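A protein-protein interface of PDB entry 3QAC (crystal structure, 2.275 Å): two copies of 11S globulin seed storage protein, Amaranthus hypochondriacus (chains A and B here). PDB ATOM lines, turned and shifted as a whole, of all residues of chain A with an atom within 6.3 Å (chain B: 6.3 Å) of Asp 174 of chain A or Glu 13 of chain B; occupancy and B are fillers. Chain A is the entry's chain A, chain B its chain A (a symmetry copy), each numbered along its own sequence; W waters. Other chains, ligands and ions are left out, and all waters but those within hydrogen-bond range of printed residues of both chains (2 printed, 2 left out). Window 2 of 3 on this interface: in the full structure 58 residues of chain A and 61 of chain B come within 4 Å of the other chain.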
ATOM      1  N   SER A  69     -18.518  15.227  12.303  1.00  0.00           N
ATOM      2  CA  SER A  69     -18.130  15.065  10.914  1.00  0.00           C
ATOM      3  C   SER A  69     -17.479  16.317  10.352  1.00  0.00           C
ATOM      4  O   SER A  69     -16.846  16.260   9.307  1.00  0.00           O
ATOM      5  CB  SER A  69     -19.360  14.728  10.070  1.00  0.00           C
ATOM      6  OG  SER A  69     -20.305  15.775  10.175  1.00  0.00           O
ATOM      7  N   THR A 166     -19.322  23.301   9.216  1.00  0.00           N
ATOM      8  CA  THR A 166     -20.200  22.290   8.662  1.00  0.00           C
ATOM      9  C   THR A 166     -20.119  22.297   7.150  1.00  0.00           C
ATOM     10  O   THR A 166     -20.329  21.275   6.520  1.00  0.00           O
ATOM     11  CB  THR A 166     -21.643  22.542   9.100  1.00  0.00           C
ATOM     12  OG1 THR A 166     -21.924  23.932   8.966  1.00  0.00           O
ATOM     13  CG2 THR A 166     -21.820  22.187  10.551  1.00  0.00           C
ATOM     14  N   ASN A 171     -16.731  17.659   5.811  1.00  0.00           N
ATOM     15  CA  ASN A 171     -18.034  17.218   6.292  1.00  0.00           C
ATOM     16  C   ASN A 171     -18.907  16.716   5.144  1.00  0.00           C
ATOM     17  O   ASN A 171     -19.335  17.499   4.300  1.00  0.00           O
ATOM     18  CB  ASN A 171     -18.779  18.335   7.033  1.00  0.00           C
ATOM     19  CG  ASN A 171     -20.218  17.920   7.404  1.00  0.00           C
ATOM     20  OD1 ASN A 171     -20.478  16.761   7.710  1.00  0.00           O
ATOM     21  ND2 ASN A 171     -21.144  18.860   7.339  1.00  0.00           N
ATOM     22  N   GLN A 172     -19.163  15.413   5.113  1.00  0.00           N
ATOM     23  CA  GLN A 172     -19.969  14.841   4.045  1.00  0.00           C
ATOM     24  C   GLN A 172     -21.402  14.489   4.497  1.00  0.00           C
ATOM     25  O   GLN A 172     -22.158  13.873   3.760  1.00  0.00           O
ATOM     26  CB  GLN A 172     -19.254  13.637   3.431  1.00  0.00           C
ATOM     27  CG  GLN A 172     -17.846  13.976   2.891  1.00  0.00           C
ATOM     28  CD  GLN A 172     -17.279  12.878   2.007  1.00  0.00           C
ATOM     29  OE1 GLN A 172     -16.191  13.001   1.438  1.00  0.00           O
ATOM     30  NE2 GLN A 172     -18.004  11.794   1.904  1.00  0.00           N
ATOM     31  N   LEU A 173     -21.759  14.868   5.717  1.00  0.00           N
ATOM     32  CA  LEU A 173     -23.128  14.698   6.198  1.00  0.00           C
ATOM     33  C   LEU A 173     -23.892  15.983   5.908  1.00  0.00           C
ATOM     34  O   LEU A 173     -23.506  16.729   5.041  1.00  0.00           O
ATOM     35  CB  LEU A 173     -23.138  14.385   7.688  1.00  0.00           C
ATOM     36  CG  LEU A 173     -22.379  13.107   8.067  1.00  0.00           C
ATOM     37  CD1 LEU A 173     -22.166  13.014   9.575  1.00  0.00           C
ATOM     38  CD2 LEU A 173     -23.114  11.888   7.552  1.00  0.00           C
ATOM     39  N   ASP A 174     -24.989  16.248   6.606  1.00  0.00           N
ATOM     40  CA  ASP A 174     -25.752  17.458   6.305  1.00  0.00           C
ATOM     41  C   ASP A 174     -24.972  18.747   6.611  1.00  0.00           C
ATOM     42  O   ASP A 174     -24.082  18.773   7.459  1.00  0.00           O
ATOM     43  CB  ASP A 174     -27.082  17.465   7.053  1.00  0.00           C
ATOM     44  CG  ASP A 174     -28.066  16.418   6.537  1.00  0.00           C
ATOM     45  OD1 ASP A 174     -28.962  16.064   7.324  1.00  0.00           O
ATOM     46  OD2 ASP A 174     -27.959  15.946   5.377  1.00  0.00           O
ATOM     47  N   LYS A 175     -25.352  19.818   5.927  1.00  0.00           N
ATOM     48  CA  LYS A 175     -24.672  21.100   6.009  1.00  0.00           C
ATOM     49  C   LYS A 175     -25.402  22.077   6.920  1.00  0.00           C
ATOM     50  O   LYS A 175     -24.844  23.082   7.354  1.00  0.00           O
ATOM     51  CB  LYS A 175     -24.561  21.711   4.609  1.00  0.00           C
ATOM     52  CG  LYS A 175     -23.754  20.854   3.639  1.00  0.00           C
ATOM     53  CD  LYS A 175     -22.381  20.543   4.220  1.00  0.00           C
ATOM     54  CE  LYS A 175     -21.481  19.846   3.200  1.00  0.00           C
ATOM     55  NZ  LYS A 175     -20.023  20.027   3.536  1.00  0.00           N
ATOM     56  N   ASN A 176     -26.661  21.778   7.200  1.00  0.00           N
ATOM     57  CA  ASN A 176     -27.475  22.633   8.053  1.00  0.00           C
ATOM     58  C   ASN A 176     -26.996  22.737   9.500  1.00  0.00           C
ATOM     59  O   ASN A 176     -26.896  23.838  10.037  1.00  0.00           O
ATOM     60  CB  ASN A 176     -28.944  22.204   7.982  1.00  0.00           C
ATOM     61  CG  ASN A 176     -29.535  22.415   6.590  1.00  0.00           C
ATOM     62  OD1 ASN A 176     -28.840  22.867   5.667  1.00  0.00           O
ATOM     63  ND2 ASN A 176     -30.818  22.086   6.430  1.00  0.00           N
ATOM     64  N   PHE A 177     -26.704  21.596  10.119  1.00  0.00           N
ATOM     65  CA  PHE A 177     -26.320  21.555  11.530  1.00  0.00           C
ATOM     66  C   PHE A 177     -25.154  20.597  11.752  1.00  0.00           C
ATOM     67  O   PHE A 177     -25.024  19.602  11.051  1.00  0.00           O
ATOM     68  CB  PHE A 177     -27.512  21.107  12.401  1.00  0.00           C
ATOM     69  CG  PHE A 177     -28.729  21.983  12.258  1.00  0.00           C
ATOM     70  CD1 PHE A 177     -28.903  23.096  13.080  1.00  0.00           C
ATOM     71  CD2 PHE A 177     -29.693  21.704  11.290  1.00  0.00           C
ATOM     72  CE1 PHE A 177     -30.012  23.916  12.943  1.00  0.00           C
ATOM     73  CE2 PHE A 177     -30.807  22.519  11.140  1.00  0.00           C
ATOM     74  CZ  PHE A 177     -30.973  23.625  11.970  1.00  0.00           C
ATOM     75  N   PRO A 178     -24.309  20.878  12.748  1.00  0.00           N
ATOM     76  CA  PRO A 178     -23.258  19.899  13.048  1.00  0.00           C
ATOM     77  C   PRO A 178     -23.893  18.574  13.426  1.00  0.00           C
ATOM     78  O   PRO A 178     -25.010  18.536  13.946  1.00  0.00           O
ATOM     79  CB  PRO A 178     -22.554  20.502  14.261  1.00  0.00           C
ATOM     80  CG  PRO A 178     -22.755  21.971  14.107  1.00  0.00           C
ATOM     81  CD  PRO A 178     -24.158  22.108  13.541  1.00  0.00           C
ATOM     82  N   THR A 179     -23.197  17.493  13.123  1.00  0.00           N
ATOM     83  CA  THR A 179     -23.593  16.189  13.592  1.00  0.00           C
ATOM     84  C   THR A 179     -22.536  15.754  14.583  1.00  0.00           C
ATOM     85  O   THR A 179     -21.343  15.697  14.256  1.00  0.00           O
ATOM     86  CB  THR A 179     -23.678  15.204  12.445  1.00  0.00           C
ATOM     87  OG1 THR A 179     -24.712  15.628  11.550  1.00  0.00           O
ATOM     88  CG2 THR A 179     -24.021  13.833  12.944  1.00  0.00           C
ATOM     89  N   GLN B  10     -33.642  21.718   0.783  1.00  0.00           N
ATOM     90  CA  GLN B  10     -33.899  20.709   1.810  1.00  0.00           C
ATOM     91  C   GLN B  10     -32.636  20.339   2.589  1.00  0.00           C
ATOM     92  O   GLN B  10     -32.488  20.717   3.756  1.00  0.00           O
ATOM     93  CB  GLN B  10     -34.521  19.455   1.196  1.00  0.00           C
ATOM     94  CG  GLN B  10     -36.010  19.566   0.928  1.00  0.00           C
ATOM     95  CD  GLN B  10     -36.637  18.217   0.650  1.00  0.00           C
ATOM     96  OE1 GLN B  10     -36.025  17.174   0.893  1.00  0.00           O
ATOM     97  NE2 GLN B  10     -37.864  18.228   0.139  1.00  0.00           N
ATOM     98  N   GLY B  11     -31.741  19.594   1.942  1.00  0.00           N
ATOM     99  CA  GLY B  11     -30.456  19.266   2.528  1.00  0.00           C
ATOM    100  C   GLY B  11     -30.550  18.500   3.833  1.00  0.00           C
ATOM    101  O   GLY B  11     -29.819  18.782   4.788  1.00  0.00           O
ATOM    102  N   ASN B  12     -31.454  17.526   3.883  1.00  0.00           N
ATOM    103  CA  ASN B  12     -31.573  16.682   5.066  1.00  0.00           C
ATOM    104  C   ASN B  12     -31.434  15.212   4.766  1.00  0.00           C
ATOM    105  O   ASN B  12     -31.862  14.365   5.549  1.00  0.00           O
ATOM    106  CB  ASN B  12     -32.895  16.942   5.771  1.00  0.00           C
ATOM    107  CG  ASN B  12     -32.847  18.177   6.620  1.00  0.00           C
ATOM    108  OD1 ASN B  12     -33.283  19.250   6.199  1.00  0.00           O
ATOM    109  ND2 ASN B  12     -32.280  18.047   7.821  1.00  0.00           N
ATOM    110  N   GLU B  13     -30.840  14.903   3.623  1.00  0.00           N
ATOM    111  CA  GLU B  13     -30.737  13.513   3.206  1.00  0.00           C
ATOM    112  C   GLU B  13     -29.836  12.676   4.113  1.00  0.00           C
ATOM    113  O   GLU B  13     -29.929  11.451   4.092  1.00  0.00           O
ATOM    114  CB  GLU B  13     -30.303  13.407   1.751  1.00  0.00           C
ATOM    115  CG  GLU B  13     -29.324  14.471   1.367  1.00  0.00           C
ATOM    116  CD  GLU B  13     -30.016  15.765   1.067  1.00  0.00           C
ATOM    117  OE1 GLU B  13     -31.028  15.723   0.332  1.00  0.00           O
ATOM    118  OE2 GLU B  13     -29.550  16.812   1.562  1.00  0.00           O
ATOM    119  N   CYS B  14     -28.992  13.317   4.925  1.00  0.00           N
ATOM    120  CA  CYS B  14     -28.172  12.550   5.863  1.00  0.00           C
ATOM    121  C   CYS B  14     -28.756  12.424   7.266  1.00  0.00           C
ATOM    122  O   CYS B  14     -28.140  11.806   8.122  1.00  0.00           O
ATOM    123  CB  CYS B  14     -26.735  13.086   5.922  1.00  0.00           C
ATOM    124  SG  CYS B  14     -25.862  12.887   4.378  1.00  0.00           S
ATOM    125  N   GLN B  15     -29.931  13.009   7.503  1.00  0.00           N
ATOM    126  CA  GLN B  15     -30.706  12.722   8.709  1.00  0.00           C
ATOM    127  C   GLN B  15     -31.302  11.333   8.548  1.00  0.00           C
ATOM    128  O   GLN B  15     -32.457  11.177   8.199  1.00  0.00           O
ATOM    129  CB  GLN B  15     -31.853  13.713   8.866  1.00  0.00           C
ATOM    130  CG  GLN B  15     -31.407  15.148   8.981  1.00  0.00           C
ATOM    131  CD  GLN B  15     -30.594  15.376  10.223  1.00  0.00           C
ATOM    132  OE1 GLN B  15     -29.375  15.200  10.222  1.00  0.00           O
ATOM    133  NE2 GLN B  15     -31.262  15.766  11.303  1.00  0.00           N
ATOM    134  N   ILE B  16     -30.500  10.321   8.808  1.00  0.00           N
ATOM    135  CA  ILE B  16     -30.881   8.967   8.524  1.00  0.00           C
ATOM    136  C   ILE B  16     -31.197   8.194   9.800  1.00  0.00           C
ATOM    137  O   ILE B  16     -30.389   8.162  10.733  1.00  0.00           O
ATOM    138  CB  ILE B  16     -29.763   8.301   7.727  1.00  0.00           C
ATOM    139  CG1 ILE B  16     -29.836   8.782   6.278  1.00  0.00           C
ATOM    140  CG2 ILE B  16     -29.826   6.784   7.837  1.00  0.00           C
ATOM    141  CD1 ILE B  16     -28.625   8.433   5.510  1.00  0.00           C
ATOM    142  N   GLN B  43     -32.516   7.374  -0.034  1.00  0.00           N
ATOM    143  CA  GLN B  43     -32.027   8.461   0.780  1.00  0.00           C
ATOM    144  C   GLN B  43     -30.528   8.349   1.058  1.00  0.00           C
ATOM    145  O   GLN B  43     -29.806   9.342   0.996  1.00  0.00           O
ATOM    146  CB  GLN B  43     -32.773   8.510   2.107  1.00  0.00           C
ATOM    147  CG  GLN B  43     -32.348   9.668   2.959  1.00  0.00           C
ATOM    148  CD  GLN B  43     -33.155   9.790   4.215  1.00  0.00           C
ATOM    149  OE1 GLN B  43     -34.248   9.221   4.326  1.00  0.00           O
ATOM    150  NE2 GLN B  43     -32.632  10.537   5.179  1.00  0.00           N
ATOM    151  N   GLU B  44     -30.067   7.155   1.403  1.00  0.00           N
ATOM    152  CA  GLU B  44     -28.677   7.025   1.797  1.00  0.00           C
ATOM    153  C   GLU B  44     -27.744   7.197   0.597  1.00  0.00           C
ATOM    154  O   GLU B  44     -26.598   7.578   0.782  1.00  0.00           O
ATOM    155  CB  GLU B  44     -28.396   5.732   2.580  1.00  0.00           C
ATOM    156  CG  GLU B  44     -28.754   4.438   1.867  1.00  0.00           C
ATOM    157  CD  GLU B  44     -30.201   3.997   2.141  1.00  0.00           C
ATOM    158  OE1 GLU B  44     -31.135   4.814   1.926  1.00  0.00           O
ATOM    159  OE2 GLU B  44     -30.398   2.836   2.579  1.00  0.00           O
ATOM    160  N   ARG B  46     -28.485   9.425  -1.743  1.00  0.00           N
ATOM    161  CA  ARG B  46     -28.527  10.864  -1.907  1.00  0.00           C
ATOM    162  C   ARG B  46     -27.560  11.480  -0.898  1.00  0.00           C
ATOM    163  O   ARG B  46     -26.804  12.389  -1.221  1.00  0.00           O
ATOM    164  CB  ARG B  46     -29.964  11.397  -1.728  1.00  0.00           C
ATOM    165  CG  ARG B  46     -30.904  10.974  -2.857  1.00  0.00           C
ATOM    166  CD  ARG B  46     -32.188  11.812  -2.914  1.00  0.00           C
ATOM    167  NE  ARG B  46     -33.182  11.334  -1.954  1.00  0.00           N
ATOM    168  CZ  ARG B  46     -33.530  12.001  -0.857  1.00  0.00           C
ATOM    169  NH1 ARG B  46     -32.963  13.187  -0.606  1.00  0.00           N
ATOM    170  NH2 ARG B  46     -34.442  11.492  -0.020  1.00  0.00           N
ATOM    171  N   CYS B  47     -27.594  10.968   0.324  1.00  0.00           N
ATOM    172  CA  CYS B  47     -26.694  11.406   1.367  1.00  0.00           C
ATOM    173  C   CYS B  47     -25.224  11.203   0.951  1.00  0.00           C
ATOM    174  O   CYS B  47     -24.396  12.086   1.151  1.00  0.00           O
ATOM    175  CB  CYS B  47     -26.981  10.632   2.654  1.00  0.00           C
ATOM    176  SG  CYS B  47     -25.758  10.918   3.959  1.00  0.00           S
HETATM  177  O   HOH W   1     -29.511  18.612   7.986  1.00  0.00           O
HETATM  178  O   HOH W   2     -27.505  19.715   4.333  1.00  0.00           O
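Of the 11 printed residues of chain A, 4 touch a printed residue of chain B.
Printed residues of chain B that touch a printed residue of chain A: Gln 10, Gly 11, Asn 12, Glu 13, Cys 14, Gln 15 and Cys 47.
Along chain B the printed residues that touch a printed residue of chain A span positions 10 to 47.
Among the printed residues, no Asp or Glu carboxylate lies within 4 Å of a Lys or Arg side-chain nitrogen of the other chain.
The side-chain amide oxygen of Asn 171 of chain A sits at hydrogen-bond distance from the backbone NH of Leu 173 of chain A, 3.0 Å away.
ND2 of Asn 171 of chain A is in hydrogen-bond range of O of Asp 174 of chain A (2.9 Å).
The backbone carbonyl oxygen (O) of Glu 13 of chain B lies within hydrogen-bond range of the side-chain amide nitrogen (NE2) of Gln 43 of chain B (3.1 Å).
The side-chain carboxylate (OE1) of Glu 13 of chain B is in salt-bridge range of the guanidinium group (NH1) of Arg 46 of chain B (3.3 Å).
SG of Cys 47 of chain B is disulfide-bonded to SG of Cys 14 of chain B (2.0 Å).
O of Gln 15 of chain B sits at hydrogen-bond distance from NE2 of Gln 43 of chain B.
Among the printed residues, merely in contact across the chains: Gln 172 of chain A with Cys 14 of chain B, Gln 172 of chain A with Cys 47 of chain B, Leu 173 of chain A with Cys 14 of chain B, Asp 174 of chain A with Asn 12 of chain B, Asp 174 of chain A with Glu 13 of chain B, Asn 176 of chain A with Gly 11 of chain B and Asn 176 of chain A with Asn 12 of chain B.
Printed residues of chain B within 4 Å of Gln 172 of chain A: Cys 14 (3.9 Å) and Cys 47 (3.9 Å).
Of the printed residues of chain A, Gln 10 of chain B touches Asn 176 (3.4 Å).
Of the printed residues of chain A, Gly 11 of chain B touches Asp 174 (3.4 Å) and Asn 176 (3.8 Å).
Printed residues of chain A within 4 Å of Asn 12 of chain B: Asp 174 (3.5 Å) and Asn 176 (3.8 Å).
Of chain A, only Asp 174 comes within 4 Å of Glu 13 of chain B.
Ile 16 of chain B touches none of the printed residues of chain A.
Printed residues of chain A within 4 Å of Cys 47 of chain B: Gln 172.
The nearest residue of chain B that does not touch Asp 174 of chain A is Cys 47 of chain B (5.7 Å).
Water W2 bridges the backbone carbonyl oxygen of Gly 11 of chain B and the backbone NH of Lys 175 of chain A.
Water W1 lies within hydrogen-bond range of the side-chain carboxylate of Asp 174 of chain A, the side-chain amide nitrogen of Asn 12 of chain B and the backbone carbonyl oxygen of Gly 11 of chain B.
The side-chain carboxylate of Asp 174 of chain A lies within hydrogen-bond range of the backbone NH of Cys 14 of chain B, 2.9 Å away.
OD1 of Asp 174 of chain A sits close to OE1 of Gln 15 of chain B.
ND2 of Asn 176 of chain A sits at hydrogen-bond distance from O of Gln 10 of chain B (3.4 Å).
The side-chain carboxylate of Asp 174 of chain A sits close to the backbone carbonyl oxygen of Gly 11 of chain B.
No position is printed for both chains.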
